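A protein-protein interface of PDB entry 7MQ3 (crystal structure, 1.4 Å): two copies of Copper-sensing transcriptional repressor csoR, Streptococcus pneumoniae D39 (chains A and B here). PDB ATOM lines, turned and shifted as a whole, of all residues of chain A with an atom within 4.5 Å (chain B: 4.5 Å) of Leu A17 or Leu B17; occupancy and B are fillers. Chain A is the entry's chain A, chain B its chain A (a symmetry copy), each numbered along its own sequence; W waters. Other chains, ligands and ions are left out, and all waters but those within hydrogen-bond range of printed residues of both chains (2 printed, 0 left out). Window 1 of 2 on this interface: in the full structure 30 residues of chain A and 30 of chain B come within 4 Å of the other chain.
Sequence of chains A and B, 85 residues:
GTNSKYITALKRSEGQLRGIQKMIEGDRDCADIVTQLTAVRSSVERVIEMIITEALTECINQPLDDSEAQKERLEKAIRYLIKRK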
ATOM      1  N   LEU A  10      25.230 -11.484  21.775  1.00  0.00           N
ATOM      2  CA  LEU A  10      24.483 -11.917  22.951  1.00  0.00           C
ATOM      3  C   LEU A  10      23.392 -12.917  22.585  1.00  0.00           C
ATOM      4  O   LEU A  10      23.048 -13.780  23.400  1.00  0.00           O
ATOM      5  CB  LEU A  10      23.883 -10.709  23.663  1.00  0.00           C
ATOM      6  CG  LEU A  10      24.905  -9.714  24.214  1.00  0.00           C
ATOM      7  CD1 LEU A  10      24.196  -8.508  24.816  1.00  0.00           C
ATOM      8  CD2 LEU A  10      25.809 -10.361  25.248  1.00  0.00           C
ATOM      9  N   SER A  13      25.124 -16.174  22.670  1.00  0.00           N
ATOM     10  CA  SER A  13      25.262 -16.651  24.042  1.00  0.00           C
ATOM     11  C   SER A  13      23.924 -17.117  24.600  1.00  0.00           C
ATOM     12  O   SER A  13      23.857 -18.112  25.331  1.00  0.00           O
ATOM     13  CB  SER A  13      25.850 -15.546  24.915  1.00  0.00           C
ATOM     14  OG  SER A  13      27.170 -15.234  24.509  1.00  0.00           O
ATOM     15  N   GLU A  14      22.847 -16.406  24.263  1.00  0.00           N
ATOM     16  CA  GLU A  14      21.509 -16.828  24.663  1.00  0.00           C
ATOM     17  C   GLU A  14      21.209 -18.233  24.163  1.00  0.00           C
ATOM     18  O   GLU A  14      20.736 -19.088  24.922  1.00  0.00           O
ATOM     19  CB  GLU A  14      20.495 -15.829  24.107  1.00  0.00           C
ATOM     20  CG  GLU A  14      19.059 -16.086  24.483  1.00  0.00           C
ATOM     21  CD  GLU A  14      18.090 -15.278  23.633  1.00  0.00           C
ATOM     22  OE1 GLU A  14      18.507 -14.255  23.048  1.00  0.00           O
ATOM     23  OE2 GLU A  14      16.908 -15.668  23.546  1.00  0.00           O
ATOM     24  N   GLY A  15      21.476 -18.496  22.887  1.00  0.00           N
ATOM     25  CA  GLY A  15      21.233 -19.827  22.359  1.00  0.00           C
ATOM     26  C   GLY A  15      22.128 -20.874  22.991  1.00  0.00           C
ATOM     27  O   GLY A  15      21.696 -22.001  23.251  1.00  0.00           O
ATOM     28  N   GLN A  16      23.389 -20.521  23.241  1.00  0.00           N
ATOM     29  CA  GLN A  16      24.301 -21.460  23.879  1.00  0.00           C
ATOM     30  C   GLN A  16      23.820 -21.823  25.275  1.00  0.00           C
ATOM     31  O   GLN A  16      23.934 -22.979  25.700  1.00  0.00           O
ATOM     32  CB  GLN A  16      25.702 -20.857  23.943  1.00  0.00           C
ATOM     33  CG  GLN A  16      26.469 -20.923  22.636  1.00  0.00           C
ATOM     34  CD  GLN A  16      27.718 -20.065  22.656  1.00  0.00           C
ATOM     35  OE1 GLN A  16      27.879 -19.167  21.832  1.00  0.00           O
ATOM     36  NE2 GLN A  16      28.608 -20.335  23.604  1.00  0.00           N
ATOM     37  N   LEU A  17      23.285 -20.848  26.010  1.00  0.00           N
ATOM     38  CA  LEU A  17      22.727 -21.145  27.323  1.00  0.00           C
ATOM     39  C   LEU A  17      21.586 -22.146  27.218  1.00  0.00           C
ATOM     40  O   LEU A  17      21.437 -23.018  28.077  1.00  0.00           O
ATOM     41  CB  LEU A  17      22.247 -19.858  27.989  1.00  0.00           C
ATOM     42  CG  LEU A  17      23.328 -18.992  28.638  1.00  0.00           C
ATOM     43  CD1 LEU A  17      22.719 -17.698  29.164  1.00  0.00           C
ATOM     44  CD2 LEU A  17      24.034 -19.742  29.751  1.00  0.00           C
ATOM     45  N   ARG A  18      20.773 -22.043  26.165  1.00  0.00           N
ATOM     46  CA  ARG A  18      19.719 -23.030  25.959  1.00  0.00           C
ATOM     47  C   ARG A  18      20.308 -24.414  25.727  1.00  0.00           C
ATOM     48  O   ARG A  18      19.821 -25.409  26.280  1.00  0.00           O
ATOM     49  CB  ARG A  18      18.844 -22.620  24.777  1.00  0.00           C
ATOM     50  CG  ARG A  18      17.785 -21.584  25.113  1.00  0.00           C
ATOM     51  CD  ARG A  18      16.731 -21.524  24.019  1.00  0.00           C
ATOM     52  NE  ARG A  18      17.226 -20.868  22.813  1.00  0.00           N
ATOM     53  CZ  ARG A  18      17.297 -19.549  22.656  1.00  0.00           C
ATOM     54  NH1 ARG A  18      16.918 -18.734  23.638  1.00  0.00           N
ATOM     55  NH2 ARG A  18      17.754 -19.035  21.521  1.00  0.00           N
ATOM     56  N   GLY A  19      21.359 -24.501  24.913  1.00  0.00           N
ATOM     57  CA  GLY A  19      22.035 -25.771  24.736  1.00  0.00           C
ATOM     58  C   GLY A  19      22.574 -26.330  26.039  1.00  0.00           C
ATOM     59  O   GLY A  19      22.486 -27.532  26.294  1.00  0.00           O
ATOM     60  N   ILE A  20      23.146 -25.464  26.876  1.00  0.00           N
ATOM     61  CA  ILE A  20      23.720 -25.934  28.132  1.00  0.00           C
ATOM     62  C   ILE A  20      22.624 -26.427  29.064  1.00  0.00           C
ATOM     63  O   ILE A  20      22.812 -27.398  29.805  1.00  0.00           O
ATOM     64  CB  ILE A  20      24.577 -24.834  28.781  1.00  0.00           C
ATOM     65  CG1 ILE A  20      25.783 -24.525  27.894  1.00  0.00           C
ATOM     66  CG2 ILE A  20      25.031 -25.269  30.168  1.00  0.00           C
ATOM     67  CD1 ILE A  20      26.461 -23.221  28.218  1.00  0.00           C
ATOM     68  N   GLN A  21      21.464 -25.767  29.047  1.00  0.00           N
ATOM     69  CA  GLN A  21      20.326 -26.264  29.811  1.00  0.00           C
ATOM     70  C   GLN A  21      19.994 -27.698  29.424  1.00  0.00           C
ATOM     71  O   GLN A  21      19.683 -28.527  30.286  1.00  0.00           O
ATOM     72  CB  GLN A  21      19.116 -25.358  29.592  1.00  0.00           C
ATOM     73  CG  GLN A  21      19.261 -23.963  30.173  1.00  0.00           C
ATOM     74  CD  GLN A  21      18.279 -22.983  29.559  1.00  0.00           C
ATOM     75  OE1 GLN A  21      17.168 -23.354  29.182  1.00  0.00           O
ATOM     76  NE2 GLN A  21      18.687 -21.724  29.455  1.00  0.00           N
ATOM     77  N   LEU A  37      29.822 -23.392  29.572  1.00  0.00           N
ATOM     78  CA  LEU A  37      29.500 -22.235  30.398  1.00  0.00           C
ATOM     79  C   LEU A  37      30.647 -21.233  30.414  1.00  0.00           C
ATOM     80  O   LEU A  37      30.417 -20.019  30.421  1.00  0.00           O
ATOM     81  CB  LEU A  37      29.162 -22.681  31.818  1.00  0.00           C
ATOM     82  CG  LEU A  37      27.768 -23.272  32.013  1.00  0.00           C
ATOM     83  CD1 LEU A  37      27.666 -23.911  33.394  1.00  0.00           C
ATOM     84  CD2 LEU A  37      26.700 -22.215  31.831  1.00  0.00           C
ATOM     85  N   VAL A  40      30.462 -19.135  27.299  1.00  0.00           N
ATOM     86  CA  VAL A  40      29.446 -18.098  27.436  1.00  0.00           C
ATOM     87  C   VAL A  40      29.967 -16.963  28.306  1.00  0.00           C
ATOM     88  O   VAL A  40      29.827 -15.783  27.968  1.00  0.00           O
ATOM     89  CB  VAL A  40      28.139 -18.688  27.995  1.00  0.00           C
ATOM     90  CG1 VAL A  40      27.181 -17.563  28.382  1.00  0.00           C
ATOM     91  CG2 VAL A  40      27.499 -19.615  26.979  1.00  0.00           C
ATOM     92  N   LEU B  10      20.159 -20.733  34.619  1.00  0.00           N
ATOM     93  CA  LEU B  10      20.611 -20.361  33.282  1.00  0.00           C
ATOM     94  C   LEU B  10      19.467 -19.825  32.432  1.00  0.00           C
ATOM     95  O   LEU B  10      19.692 -18.986  31.553  1.00  0.00           O
ATOM     96  CB  LEU B  10      21.268 -21.558  32.601  1.00  0.00           C
ATOM     97  CG  LEU B  10      22.528 -22.080  33.291  1.00  0.00           C
ATOM     98  CD1 LEU B  10      23.040 -23.327  32.582  1.00  0.00           C
ATOM     99  CD2 LEU B  10      23.615 -21.022  33.340  1.00  0.00           C
ATOM    100  N   SER B  13      19.384 -16.226  33.244  1.00  0.00           N
ATOM    101  CA  SER B  13      20.420 -15.505  32.510  1.00  0.00           C
ATOM    102  C   SER B  13      20.067 -15.390  31.033  1.00  0.00           C
ATOM    103  O   SER B  13      20.321 -14.356  30.404  1.00  0.00           O
ATOM    104  CB  SER B  13      21.761 -16.212  32.687  1.00  0.00           C
ATOM    105  OG  SER B  13      22.180 -16.163  34.038  1.00  0.00           O
ATOM    106  N   GLU B  14      19.481 -16.445  30.466  1.00  0.00           N
ATOM    107  CA  GLU B  14      19.015 -16.397  29.084  1.00  0.00           C
ATOM    108  C   GLU B  14      18.026 -15.258  28.884  1.00  0.00           C
ATOM    109  O   GLU B  14      18.145 -14.476  27.932  1.00  0.00           O
ATOM    110  CB  GLU B  14      18.371 -17.739  28.739  1.00  0.00           C
ATOM    111  CG  GLU B  14      17.888 -17.879  27.319  1.00  0.00           C
ATOM    112  CD  GLU B  14      16.968 -19.078  27.142  1.00  0.00           C
ATOM    113  OE1 GLU B  14      17.015 -20.005  27.979  1.00  0.00           O
ATOM    114  OE2 GLU B  14      16.193 -19.094  26.164  1.00  0.00           O
ATOM    115  N   GLY B  15      17.040 -15.144  29.769  1.00  0.00           N
ATOM    116  CA  GLY B  15      16.079 -14.062  29.642  1.00  0.00           C
ATOM    117  C   GLY B  15      16.710 -12.699  29.840  1.00  0.00           C
ATOM    118  O   GLY B  15      16.360 -11.735  29.155  1.00  0.00           O
ATOM    119  N   GLN B  16      17.646 -12.597  30.784  1.00  0.00           N
ATOM    120  CA  GLN B  16      18.325 -11.330  31.011  1.00  0.00           C
ATOM    121  C   GLN B  16      19.110 -10.904  29.780  1.00  0.00           C
ATOM    122  O   GLN B  16      19.153  -9.715  29.442  1.00  0.00           O
ATOM    123  CB  GLN B  16      19.255 -11.449  32.216  1.00  0.00           C
ATOM    124  CG  GLN B  16      18.552 -11.371  33.557  1.00  0.00           C
ATOM    125  CD  GLN B  16      19.450 -11.784  34.705  1.00  0.00           C
ATOM    126  OE1 GLN B  16      19.139 -12.713  35.447  1.00  0.00           O
ATOM    127  NE2 GLN B  16      20.577 -11.097  34.854  1.00  0.00           N
ATOM    128  N   LEU B  17      19.744 -11.858  29.099  1.00  0.00           N
ATOM    129  CA  LEU B  17      20.443 -11.531  27.863  1.00  0.00           C
ATOM    130  C   LEU B  17      19.484 -10.966  26.827  1.00  0.00           C
ATOM    131  O   LEU B  17      19.840 -10.051  26.080  1.00  0.00           O
ATOM    132  CB  LEU B  17      21.146 -12.773  27.318  1.00  0.00           C
ATOM    133  CG  LEU B  17      22.474 -13.139  27.980  1.00  0.00           C
ATOM    134  CD1 LEU B  17      23.001 -14.451  27.409  1.00  0.00           C
ATOM    135  CD2 LEU B  17      23.495 -12.032  27.807  1.00  0.00           C
ATOM    136  N   ARG B  18      18.259 -11.491  26.771  1.00  0.00           N
ATOM    137  CA  ARG B  18      17.266 -10.927  25.863  1.00  0.00           C
ATOM    138  C   ARG B  18      16.940  -9.489  26.238  1.00  0.00           C
ATOM    139  O   ARG B  18      16.841  -8.615  25.367  1.00  0.00           O
ATOM    140  CB  ARG B  18      15.999 -11.780  25.881  1.00  0.00           C
ATOM    141  CG  ARG B  18      16.070 -13.021  25.007  1.00  0.00           C
ATOM    142  CD  ARG B  18      14.679 -13.587  24.772  1.00  0.00           C
ATOM    143  NE  ARG B  18      14.146 -14.251  25.957  1.00  0.00           N
ATOM    144  CZ  ARG B  18      14.462 -15.490  26.325  1.00  0.00           C
ATOM    145  NH1 ARG B  18      15.324 -16.205  25.605  1.00  0.00           N
ATOM    146  NH2 ARG B  18      13.924 -16.020  27.415  1.00  0.00           N
ATOM    147  N   GLY B  19      16.771  -9.219  27.532  1.00  0.00           N
ATOM    148  CA  GLY B  19      16.568  -7.851  27.967  1.00  0.00           C
ATOM    149  C   GLY B  19      17.721  -6.942  27.584  1.00  0.00           C
ATOM    150  O   GLY B  19      17.512  -5.802  27.168  1.00  0.00           O
ATOM    151  N   ILE B  20      18.951  -7.435  27.727  1.00  0.00           N
ATOM    152  CA  ILE B  20      20.110  -6.606  27.413  1.00  0.00           C
ATOM    153  C   ILE B  20      20.173  -6.327  25.920  1.00  0.00           C
ATOM    154  O   ILE B  20      20.568  -5.236  25.495  1.00  0.00           O
ATOM    155  CB  ILE B  20      21.400  -7.262  27.933  1.00  0.00           C
ATOM    156  CG1 ILE B  20      21.371  -7.327  29.459  1.00  0.00           C
ATOM    157  CG2 ILE B  20      22.618  -6.481  27.454  1.00  0.00           C
ATOM    158  CD1 ILE B  20      22.372  -8.283  30.049  1.00  0.00           C
ATOM    159  N   GLN B  21      19.790  -7.307  25.098  1.00  0.00           N
ATOM    160  CA  GLN B  21      19.696  -7.064  23.663  1.00  0.00           C
ATOM    161  C   GLN B  21      18.773  -5.890  23.368  1.00  0.00           C
ATOM    162  O   GLN B  21      19.063  -5.065  22.495  1.00  0.00           O
ATOM    163  CB  GLN B  21      19.200  -8.323  22.955  1.00  0.00           C
ATOM    164  CG  GLN B  21      20.175  -9.487  22.983  1.00  0.00           C
ATOM    165  CD  GLN B  21      19.494 -10.811  22.692  1.00  0.00           C
ATOM    166  OE1 GLN B  21      18.524 -10.871  21.937  1.00  0.00           O
ATOM    167  NE2 GLN B  21      20.000 -11.881  23.294  1.00  0.00           N
ATOM    168  N   LEU B  37      25.080  -6.856  31.996  1.00  0.00           N
ATOM    169  CA  LEU B  37      25.951  -7.899  31.467  1.00  0.00           C
ATOM    170  C   LEU B  37      26.840  -8.480  32.559  1.00  0.00           C
ATOM    171  O   LEU B  37      27.108  -9.687  32.572  1.00  0.00           O
ATOM    172  CB  LEU B  37      26.800  -7.347  30.326  1.00  0.00           C
ATOM    173  CG  LEU B  37      26.087  -7.193  28.984  1.00  0.00           C
ATOM    174  CD1 LEU B  37      26.961  -6.394  28.024  1.00  0.00           C
ATOM    175  CD2 LEU B  37      25.738  -8.544  28.397  1.00  0.00           C
ATOM    176  N   VAL B  40      24.867 -11.024  34.500  1.00  0.00           N
ATOM    177  CA  VAL B  40      24.797 -12.287  33.773  1.00  0.00           C
ATOM    178  C   VAL B  40      26.112 -13.042  33.901  1.00  0.00           C
ATOM    179  O   VAL B  40      26.133 -14.246  34.175  1.00  0.00           O
ATOM    180  CB  VAL B  40      24.423 -12.045  32.300  1.00  0.00           C
ATOM    181  CG1 VAL B  40      24.612 -13.329  31.494  1.00  0.00           C
ATOM    182  CG2 VAL B  40      22.995 -11.545  32.191  1.00  0.00           C
HETATM  183  O   HOH W   1      15.297 -22.026  27.803  1.00  0.00           O
HETATM  184  O   HOH W   2      16.889 -12.924  21.410  1.00  0.00           O
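The side-chain carboxylate (OE2) of Glu A14 lies within salt-bridge range of the guanidinium group (NH1) of Arg B18 (2.7 Å). The side-chain carboxylate of Glu A14 is in hydrogen-bond range of the side-chain amide nitrogen of Gln B21, 2.8 Å away. The side-chain carboxylate (OE2) of Glu B14 lies within salt-bridge range of the guanidinium group (NH1) of Arg A18 (2.7 Å). The side-chain carboxylate (OE1) of Glu B14 lies within hydrogen-bond range of the side-chain amide nitrogen (NE2) of Gln A21 (2.8 Å).
OE2 of Glu A14 lies within salt-bridge range of NH1 of Arg A18, at 3.1 Å. NE2 of Gln A21 sits close to O of Leu A17 (3.3 Å). The side-chain carboxylate (OE2) of Glu B14 lies within salt-bridge range of the guanidinium group (NH1) of Arg B18 (3.1 Å). O of Leu B17 lies close to NE2 of Gln B21, 3.3 Å away.
Leu A10 touches Leu B17. O of Leu A10 touches NE2 of Gln B21 (3.6 Å). Leu A10 touches Leu B37 (CD2 to CD2, 3.6 Å). Ser A13 touches Leu B17 (CB to CD1, 3.9 Å). Leu A17 touches Leu B10 (CD2 to CD2, 3.8 Å). Leu A17 touches Ser B13. CD1 of Leu A17 touches N of Glu B14, 3.7 Å away. Leu B17 touches Leu A17 (CD1 to CD1, 3.7 Å). Leu B10 touches Gln A21. CD2 of Leu A37 touches CD2 of Leu B10, at 3.6 Å.
Printed residues of chain B within 4 Å of Ser A13: Leu B17 (3.9 Å). Leu A17 touches just these residues of chain B: Leu B10 (3.8 Å), Ser B13 (3.9 Å), Glu B14 (3.7 Å) and Leu B17 (3.7 Å). Printed residues of chain B within 4 Å of Ile A20: Leu B10. Printed residues of chain A within 4 Å of Ser B13: Leu A17. Leu B17 touches just these residues of chain A: Leu A10 (3.8 Å), Ser A13 (3.9 Å), Glu A14 (3.7 Å) and Leu A17 (3.7 Å). Printed residues of chain A within 4 Å of Ile B20: Leu A10. The nearest printed residue of chain A that does not touch Leu B17 is Val A40 (5.3 Å).
Of the 12 printed residues of chain A, 8 touch a printed residue of chain B. Hydrophobic or aromatic side chains of chain A within 4 Å of the printed part of chain B: Leu A10, Leu A17, Ile A20 and Leu A37. Along chain A the printed residues that touch a printed residue of chain B span positions 10 to 37. Of the 12 printed residues of chain B, 8 touch a printed residue of chain A. Hydrophobic or aromatic side chains of chain B that line the printed part of chain A: Leu B10, Leu B17, Ile B20 and Leu B37. Among the printed residues, 19 pairs touch across the chains.
Leu A10 touches Ile B20, and with the chains exchanged Ile A20 touches Leu B10. Leu A10 touches Leu B37, and with the chains exchanged Leu A37 touches Leu B10. Glu A14 touches Gln B21, and with the chains exchanged Gln A21 touches Glu B14. Arg A18 touches its own counterpart, Arg B18. Positions printed for both chains: 10, 13, 14, 15, 16, 17, 18, 19, 20, 21, 37 and 40. Of the 19 pairs that touch across the chains among the printed residues, 19 have their exchanged pair printed and touching as well.
Water W2 lies within hydrogen-bond range of OE1 of Glu A14 and OE1 of Gln B21. Water W1 lies within hydrogen-bond range of the side-chain carboxylate of Glu B14 (2.7 Å) and the side-chain amide oxygen of Gln A21 (2.7 Å).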
